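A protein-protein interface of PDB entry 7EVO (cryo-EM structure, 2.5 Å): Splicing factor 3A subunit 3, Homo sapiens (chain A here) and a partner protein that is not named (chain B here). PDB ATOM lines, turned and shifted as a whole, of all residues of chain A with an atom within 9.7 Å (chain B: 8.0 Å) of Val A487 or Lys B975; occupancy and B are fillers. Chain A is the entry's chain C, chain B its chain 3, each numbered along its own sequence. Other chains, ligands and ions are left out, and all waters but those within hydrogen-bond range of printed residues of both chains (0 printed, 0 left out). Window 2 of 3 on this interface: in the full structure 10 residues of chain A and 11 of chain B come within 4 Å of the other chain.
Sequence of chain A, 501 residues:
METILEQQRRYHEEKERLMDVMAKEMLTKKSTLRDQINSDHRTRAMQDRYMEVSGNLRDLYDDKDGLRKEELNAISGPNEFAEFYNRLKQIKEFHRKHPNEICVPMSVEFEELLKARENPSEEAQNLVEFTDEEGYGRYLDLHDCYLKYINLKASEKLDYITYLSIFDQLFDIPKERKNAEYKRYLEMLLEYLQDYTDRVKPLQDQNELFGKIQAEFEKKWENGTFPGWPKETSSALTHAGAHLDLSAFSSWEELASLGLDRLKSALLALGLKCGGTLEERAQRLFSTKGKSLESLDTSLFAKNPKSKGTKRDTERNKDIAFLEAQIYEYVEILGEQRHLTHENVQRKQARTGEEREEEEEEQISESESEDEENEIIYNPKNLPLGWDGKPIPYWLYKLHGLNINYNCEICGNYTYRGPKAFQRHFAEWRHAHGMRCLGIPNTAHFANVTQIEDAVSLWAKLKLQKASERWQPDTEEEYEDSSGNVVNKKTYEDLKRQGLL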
ATOM      1  N   TYR A 479       7.203   8.173 -20.248  1.00  0.00           N
ATOM      2  CA  TYR A 479       6.535   9.443 -20.024  1.00  0.00           C
ATOM      3  C   TYR A 479       6.570  10.267 -21.304  1.00  0.00           C
ATOM      4  O   TYR A 479       7.526  10.182 -22.080  1.00  0.00           O
ATOM      5  CB  TYR A 479       7.198  10.207 -18.878  1.00  0.00           C
ATOM      6  N   GLU A 480       5.525  11.058 -21.523  1.00  0.00           N
ATOM      7  CA  GLU A 480       5.432  11.974 -22.660  1.00  0.00           C
ATOM      8  C   GLU A 480       5.185  13.363 -22.083  1.00  0.00           C
ATOM      9  O   GLU A 480       4.061  13.709 -21.715  1.00  0.00           O
ATOM     10  CB  GLU A 480       4.326  11.547 -23.635  1.00  0.00           C
ATOM     11  N   ASP A 481       6.250  14.154 -21.993  1.00  0.00           N
ATOM     12  CA  ASP A 481       6.166  15.452 -21.346  1.00  0.00           C
ATOM     13  C   ASP A 481       5.285  16.405 -22.153  1.00  0.00           C
ATOM     14  O   ASP A 481       5.058  16.232 -23.353  1.00  0.00           O
ATOM     15  CB  ASP A 481       7.560  16.050 -21.162  1.00  0.00           C
ATOM     16  N   SER A 482       4.789  17.435 -21.465  1.00  0.00           N
ATOM     17  CA  SER A 482       3.925  18.444 -22.065  1.00  0.00           C
ATOM     18  C   SER A 482       4.712  19.573 -22.721  1.00  0.00           C
ATOM     19  O   SER A 482       4.160  20.661 -22.938  1.00  0.00           O
ATOM     20  CB  SER A 482       2.963  19.000 -21.016  1.00  0.00           C
ATOM     21  N   SER A 483       5.990  19.349 -23.034  1.00  0.00           N
ATOM     22  CA  SER A 483       6.757  20.339 -23.780  1.00  0.00           C
ATOM     23  C   SER A 483       6.185  20.565 -25.171  1.00  0.00           C
ATOM     24  O   SER A 483       5.940  21.716 -25.549  1.00  0.00           O
ATOM     25  CB  SER A 483       8.221  19.908 -23.877  1.00  0.00           C
ATOM     26  N   GLY A 484       5.966  19.499 -25.935  1.00  0.00           N
ATOM     27  CA  GLY A 484       5.227  19.590 -27.176  1.00  0.00           C
ATOM     28  C   GLY A 484       3.818  19.069 -26.987  1.00  0.00           C
ATOM     29  O   GLY A 484       2.892  19.462 -27.703  1.00  0.00           O
ATOM     30  N   ASN A 485       3.658  18.165 -26.023  1.00  0.00           N
ATOM     31  CA  ASN A 485       2.416  17.576 -25.540  1.00  0.00           C
ATOM     32  C   ASN A 485       1.773  16.643 -26.564  1.00  0.00           C
ATOM     33  O   ASN A 485       0.756  16.025 -26.251  1.00  0.00           O
ATOM     34  CB  ASN A 485       1.375  18.627 -25.104  1.00  0.00           C
ATOM     35  N   VAL A 486       2.326  16.510 -27.769  1.00  0.00           N
ATOM     36  CA  VAL A 486       1.777  15.599 -28.766  1.00  0.00           C
ATOM     37  C   VAL A 486       2.914  14.815 -29.408  1.00  0.00           C
ATOM     38  O   VAL A 486       2.710  14.105 -30.399  1.00  0.00           O
ATOM     39  CB  VAL A 486       0.961  16.357 -29.829  1.00  0.00           C
ATOM     40  N   VAL A 487       4.117  14.943 -28.850  1.00  0.00           N
ATOM     41  CA  VAL A 487       5.302  14.293 -29.393  1.00  0.00           C
ATOM     42  C   VAL A 487       6.203  13.884 -28.238  1.00  0.00           C
ATOM     43  O   VAL A 487       5.879  14.100 -27.067  1.00  0.00           O
ATOM     44  CB  VAL A 487       6.058  15.208 -30.386  1.00  0.00           C
ATOM     45  N   ASN A 488       7.338  13.271 -28.583  1.00  0.00           N
ATOM     46  CA  ASN A 488       8.403  12.972 -27.633  1.00  0.00           C
ATOM     47  C   ASN A 488       7.939  12.072 -26.494  1.00  0.00           C
ATOM     48  O   ASN A 488       7.932  12.485 -25.330  1.00  0.00           O
ATOM     49  CB  ASN A 488       8.989  14.269 -27.067  1.00  0.00           C
ATOM     50  N   LYS A 489       7.543  10.840 -26.819  1.00  0.00           N
ATOM     51  CA  LYS A 489       7.211   9.866 -25.788  1.00  0.00           C
ATOM     52  C   LYS A 489       8.431   9.071 -25.336  1.00  0.00           C
ATOM     53  O   LYS A 489       8.283   8.151 -24.520  1.00  0.00           O
ATOM     54  CB  LYS A 489       6.118   8.907 -26.278  1.00  0.00           C
ATOM     55  N   LYS A 490       9.626   9.391 -25.838  1.00  0.00           N
ATOM     56  CA  LYS A 490      10.837   8.685 -25.442  1.00  0.00           C
ATOM     57  C   LYS A 490      11.457   9.241 -24.168  1.00  0.00           C
ATOM     58  O   LYS A 490      12.598   8.886 -23.850  1.00  0.00           O
ATOM     59  CB  LYS A 490      11.864   8.730 -26.575  1.00  0.00           C
ATOM     60  N   THR A 491      10.747  10.100 -23.441  1.00  0.00           N
ATOM     61  CA  THR A 491      11.280  10.668 -22.210  1.00  0.00           C
ATOM     62  C   THR A 491      11.316   9.610 -21.114  1.00  0.00           C
ATOM     63  O   THR A 491      10.333   8.895 -20.897  1.00  0.00           O
ATOM     64  CB  THR A 491      10.434  11.862 -21.771  1.00  0.00           C
ATOM     65  N   THR B 927      -4.866   1.230 -32.167  1.00  0.00           N
ATOM     66  CA  THR B 927      -5.795   2.019 -31.361  1.00  0.00           C
ATOM     67  C   THR B 927      -6.727   2.769 -32.297  1.00  0.00           C
ATOM     68  O   THR B 927      -6.264   3.406 -33.249  1.00  0.00           O
ATOM     69  CB  THR B 927      -5.044   2.992 -30.446  1.00  0.00           C
ATOM     70  OG1 THR B 927      -4.249   2.256 -29.513  1.00  0.00           O
ATOM     71  CG2 THR B 927      -6.018   3.863 -29.679  1.00  0.00           C
ATOM     72  N   PHE B 939      -8.217   5.236 -37.241  1.00  0.00           N
ATOM     73  CA  PHE B 939      -6.884   4.900 -36.761  1.00  0.00           C
ATOM     74  C   PHE B 939      -6.253   6.063 -36.002  1.00  0.00           C
ATOM     75  O   PHE B 939      -6.292   7.215 -36.441  1.00  0.00           O
ATOM     76  CB  PHE B 939      -6.002   4.500 -37.945  1.00  0.00           C
ATOM     77  CG  PHE B 939      -4.602   4.113 -37.568  1.00  0.00           C
ATOM     78  CD1 PHE B 939      -4.340   2.887 -36.983  1.00  0.00           C
ATOM     79  CD2 PHE B 939      -3.545   4.967 -37.820  1.00  0.00           C
ATOM     80  CE1 PHE B 939      -3.053   2.529 -36.646  1.00  0.00           C
ATOM     81  CE2 PHE B 939      -2.257   4.614 -37.482  1.00  0.00           C
ATOM     82  CZ  PHE B 939      -2.011   3.393 -36.898  1.00  0.00           C
ATOM     83  N   LEU B 940      -5.658   5.747 -34.851  1.00  0.00           N
ATOM     84  CA  LEU B 940      -4.973   6.749 -34.040  1.00  0.00           C
ATOM     85  C   LEU B 940      -3.463   6.545 -34.030  1.00  0.00           C
ATOM     86  O   LEU B 940      -2.729   7.454 -34.430  1.00  0.00           O
ATOM     87  CB  LEU B 940      -5.533   6.739 -32.614  1.00  0.00           C
ATOM     88  CG  LEU B 940      -5.134   7.925 -31.735  1.00  0.00           C
ATOM     89  CD1 LEU B 940      -5.915   9.164 -32.129  1.00  0.00           C
ATOM     90  CD2 LEU B 940      -5.351   7.604 -30.269  1.00  0.00           C
ATOM     91  N   HIS B 941      -2.971   5.380 -33.611  1.00  0.00           N
ATOM     92  CA  HIS B 941      -1.551   5.062 -33.733  1.00  0.00           C
ATOM     93  C   HIS B 941      -1.371   3.553 -33.598  1.00  0.00           C
ATOM     94  O   HIS B 941      -2.344   2.797 -33.517  1.00  0.00           O
ATOM     95  CB  HIS B 941      -0.701   5.836 -32.715  1.00  0.00           C
ATOM     96  CG  HIS B 941      -1.216   5.780 -31.310  1.00  0.00           C
ATOM     97  ND1 HIS B 941      -1.812   6.858 -30.694  1.00  0.00           N
ATOM     98  CD2 HIS B 941      -1.206   4.783 -30.395  1.00  0.00           C
ATOM     99  CE1 HIS B 941      -2.149   6.527 -29.460  1.00  0.00           C
ATOM    100  NE2 HIS B 941      -1.795   5.271 -29.256  1.00  0.00           N
ATOM    101  N   LYS B 942      -0.114   3.117 -33.559  1.00  0.00           N
ATOM    102  CA  LYS B 942       0.236   1.707 -33.652  1.00  0.00           C
ATOM    103  C   LYS B 942       1.523   1.465 -32.876  1.00  0.00           C
ATOM    104  O   LYS B 942       2.594   1.913 -33.293  1.00  0.00           O
ATOM    105  CB  LYS B 942       0.398   1.297 -35.119  1.00  0.00           C
ATOM    106  CG  LYS B 942       0.941  -0.092 -35.358  1.00  0.00           C
ATOM    107  CD  LYS B 942       1.228  -0.288 -36.839  1.00  0.00           C
ATOM    108  CE  LYS B 942       1.362  -1.754 -37.198  1.00  0.00           C
ATOM    109  NZ  LYS B 942       1.654  -1.953 -38.640  1.00  0.00           N
ATOM    110  N   THR B 943       1.415   0.757 -31.756  1.00  0.00           N
ATOM    111  CA  THR B 943       2.528   0.601 -30.831  1.00  0.00           C
ATOM    112  C   THR B 943       3.170  -0.770 -30.978  1.00  0.00           C
ATOM    113  O   THR B 943       2.487  -1.793 -30.878  1.00  0.00           O
ATOM    114  CB  THR B 943       2.065   0.790 -29.380  1.00  0.00           C
ATOM    115  OG1 THR B 943       1.530   2.109 -29.216  1.00  0.00           O
ATOM    116  CG2 THR B 943       3.222   0.600 -28.420  1.00  0.00           C
ATOM    117  N   PRO B 944       4.481  -0.822 -31.204  1.00  0.00           N
ATOM    118  CA  PRO B 944       5.169  -2.108 -31.351  1.00  0.00           C
ATOM    119  C   PRO B 944       5.507  -2.759 -30.015  1.00  0.00           C
ATOM    120  O   PRO B 944       5.814  -2.099 -29.022  1.00  0.00           O
ATOM    121  CB  PRO B 944       6.454  -1.730 -32.104  1.00  0.00           C
ATOM    122  CG  PRO B 944       6.691  -0.310 -31.753  1.00  0.00           C
ATOM    123  CD  PRO B 944       5.351   0.321 -31.529  1.00  0.00           C
ATOM    124  N   LEU B 972      -2.882   5.616 -22.197  1.00  0.00           N
ATOM    125  CA  LEU B 972      -3.005   6.186 -23.531  1.00  0.00           C
ATOM    126  C   LEU B 972      -2.112   7.411 -23.675  1.00  0.00           C
ATOM    127  O   LEU B 972      -2.068   8.270 -22.791  1.00  0.00           O
ATOM    128  CB  LEU B 972      -4.458   6.560 -23.820  1.00  0.00           C
ATOM    129  CG  LEU B 972      -4.761   6.990 -25.257  1.00  0.00           C
ATOM    130  CD1 LEU B 972      -4.315   5.924 -26.241  1.00  0.00           C
ATOM    131  CD2 LEU B 972      -6.236   7.300 -25.434  1.00  0.00           C
ATOM    132  N   GLY B 973      -1.391   7.485 -24.798  1.00  0.00           N
ATOM    133  CA  GLY B 973      -0.558   8.621 -25.112  1.00  0.00           C
ATOM    134  C   GLY B 973      -0.976   9.253 -26.431  1.00  0.00           C
ATOM    135  O   GLY B 973      -1.903   8.793 -27.108  1.00  0.00           O
ATOM    136  N   LYS B 974      -0.273  10.325 -26.790  1.00  0.00           N
ATOM    137  CA  LYS B 974      -0.583  11.036 -28.023  1.00  0.00           C
ATOM    138  C   LYS B 974       0.006  10.376 -29.260  1.00  0.00           C
ATOM    139  O   LYS B 974      -0.508  10.611 -30.358  1.00  0.00           O
ATOM    140  CB  LYS B 974      -0.098  12.483 -27.930  1.00  0.00           C
ATOM    141  CG  LYS B 974      -0.873  13.327 -26.936  1.00  0.00           C
ATOM    142  CD  LYS B 974      -1.686  14.403 -27.636  1.00  0.00           C
ATOM    143  CE  LYS B 974      -3.048  14.577 -26.981  1.00  0.00           C
ATOM    144  NZ  LYS B 974      -4.041  15.184 -27.908  1.00  0.00           N
ATOM    145  N   LYS B 975       1.054   9.563 -29.126  1.00  0.00           N
ATOM    146  CA  LYS B 975       1.675   8.948 -30.290  1.00  0.00           C
ATOM    147  C   LYS B 975       1.788   7.435 -30.150  1.00  0.00           C
ATOM    148  O   LYS B 975       2.037   6.738 -31.139  1.00  0.00           O
ATOM    149  CB  LYS B 975       3.059   9.551 -30.539  1.00  0.00           C
ATOM    150  CG  LYS B 975       3.030  10.985 -31.030  1.00  0.00           C
ATOM    151  CD  LYS B 975       3.410  11.065 -32.499  1.00  0.00           C
ATOM    152  CE  LYS B 975       4.080  12.388 -32.828  1.00  0.00           C
ATOM    153  NZ  LYS B 975       5.439  12.477 -32.236  1.00  0.00           N
ATOM    154  N   LYS B 976       1.612   6.920 -28.938  1.00  0.00           N
ATOM    155  CA  LYS B 976       1.685   5.484 -28.688  1.00  0.00           C
ATOM    156  C   LYS B 976       1.150   5.214 -27.285  1.00  0.00           C
ATOM    157  O   LYS B 976       0.672   6.130 -26.607  1.00  0.00           O
ATOM    158  CB  LYS B 976       3.123   4.972 -28.880  1.00  0.00           C
ATOM    159  CG  LYS B 976       4.122   5.527 -27.884  1.00  0.00           C
ATOM    160  CD  LYS B 976       5.444   4.790 -27.984  1.00  0.00           C
ATOM    161  CE  LYS B 976       6.404   5.219 -26.890  1.00  0.00           C
ATOM    162  NZ  LYS B 976       7.733   4.561 -27.032  1.00  0.00           N
ATOM    163  N   LEU B 977       1.222   3.962 -26.853  1.00  0.00           N
ATOM    164  CA  LEU B 977       0.839   3.575 -25.505  1.00  0.00           C
ATOM    165  C   LEU B 977       2.063   3.567 -24.598  1.00  0.00           C
ATOM    166  O   LEU B 977       3.138   3.089 -24.966  1.00  0.00           O
ATOM    167  CB  LEU B 977       0.166   2.200 -25.503  1.00  0.00           C
ATOM    168  CG  LEU B 977      -1.142   2.073 -26.285  1.00  0.00           C
ATOM    169  CD1 LEU B 977      -1.513   0.618 -26.457  1.00  0.00           C
ATOM    170  CD2 LEU B 977      -2.258   2.827 -25.588  1.00  0.00           C
ATOM    171  N   LEU B 978       1.883   4.107 -23.398  1.00  0.00           N
ATOM    172  CA  LEU B 978       2.980   4.359 -22.468  1.00  0.00           C
ATOM    173  C   LEU B 978       3.001   3.254 -21.419  1.00  0.00           C
ATOM    174  O   LEU B 978       2.023   3.061 -20.690  1.00  0.00           O
ATOM    175  CB  LEU B 978       2.830   5.734 -21.827  1.00  0.00           C
ATOM    176  CG  LEU B 978       2.754   6.903 -22.809  1.00  0.00           C
ATOM    177  CD1 LEU B 978       2.353   8.175 -22.093  1.00  0.00           C
ATOM    178  CD2 LEU B 978       4.073   7.085 -23.536  1.00  0.00           C
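Among the printed residues, pairs that only touch across the chains: Asn A485 with Lys B974 (3.2 Å), Val A486 with Lys B974 (3.7 Å), Val A486 with Lys B975 (3.2 Å), Val A487 with Lys B975 (3.4 Å), Lys A489 with Lys B976 (3.7 Å) and Lys A489 with Leu B978 (3.9 Å).
Of chain B, only Lys B975 comes within 4 Å of Val A487.
Of chain A, only Val A486 (3.2 Å) and Val A487 (3.4 Å) come within 4 Å of Lys B975.
Of the printed residues of chain A, Leu B978 touches Lys A489.
Of the printed residues of chain A, Lys B974 touches Asn A485 (3.2 Å) and Val A486 (3.7 Å).
Of the printed residues of chain B, Asn A485 touches Lys B974.
Printed residues of chain B within 4 Å of Lys A489: Lys B976 (3.7 Å) and Leu B978 (3.9 Å).
Leu B972 touches none of the printed residues of chain A.
The nearest residue of chain A that does not touch Lys B975 is Asn A488 (4.2 Å).
The nearest printed residue of chain B that does not touch Asn A485 is Gly B973 (7.0 Å).
Of the 14 printed residues of chain B, 4 touch a printed residue of chain A.
Of the 13 printed residues of chain A, 4 touch a printed residue of chain B.
Among the printed residues, 6 pairs touch across the chains.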
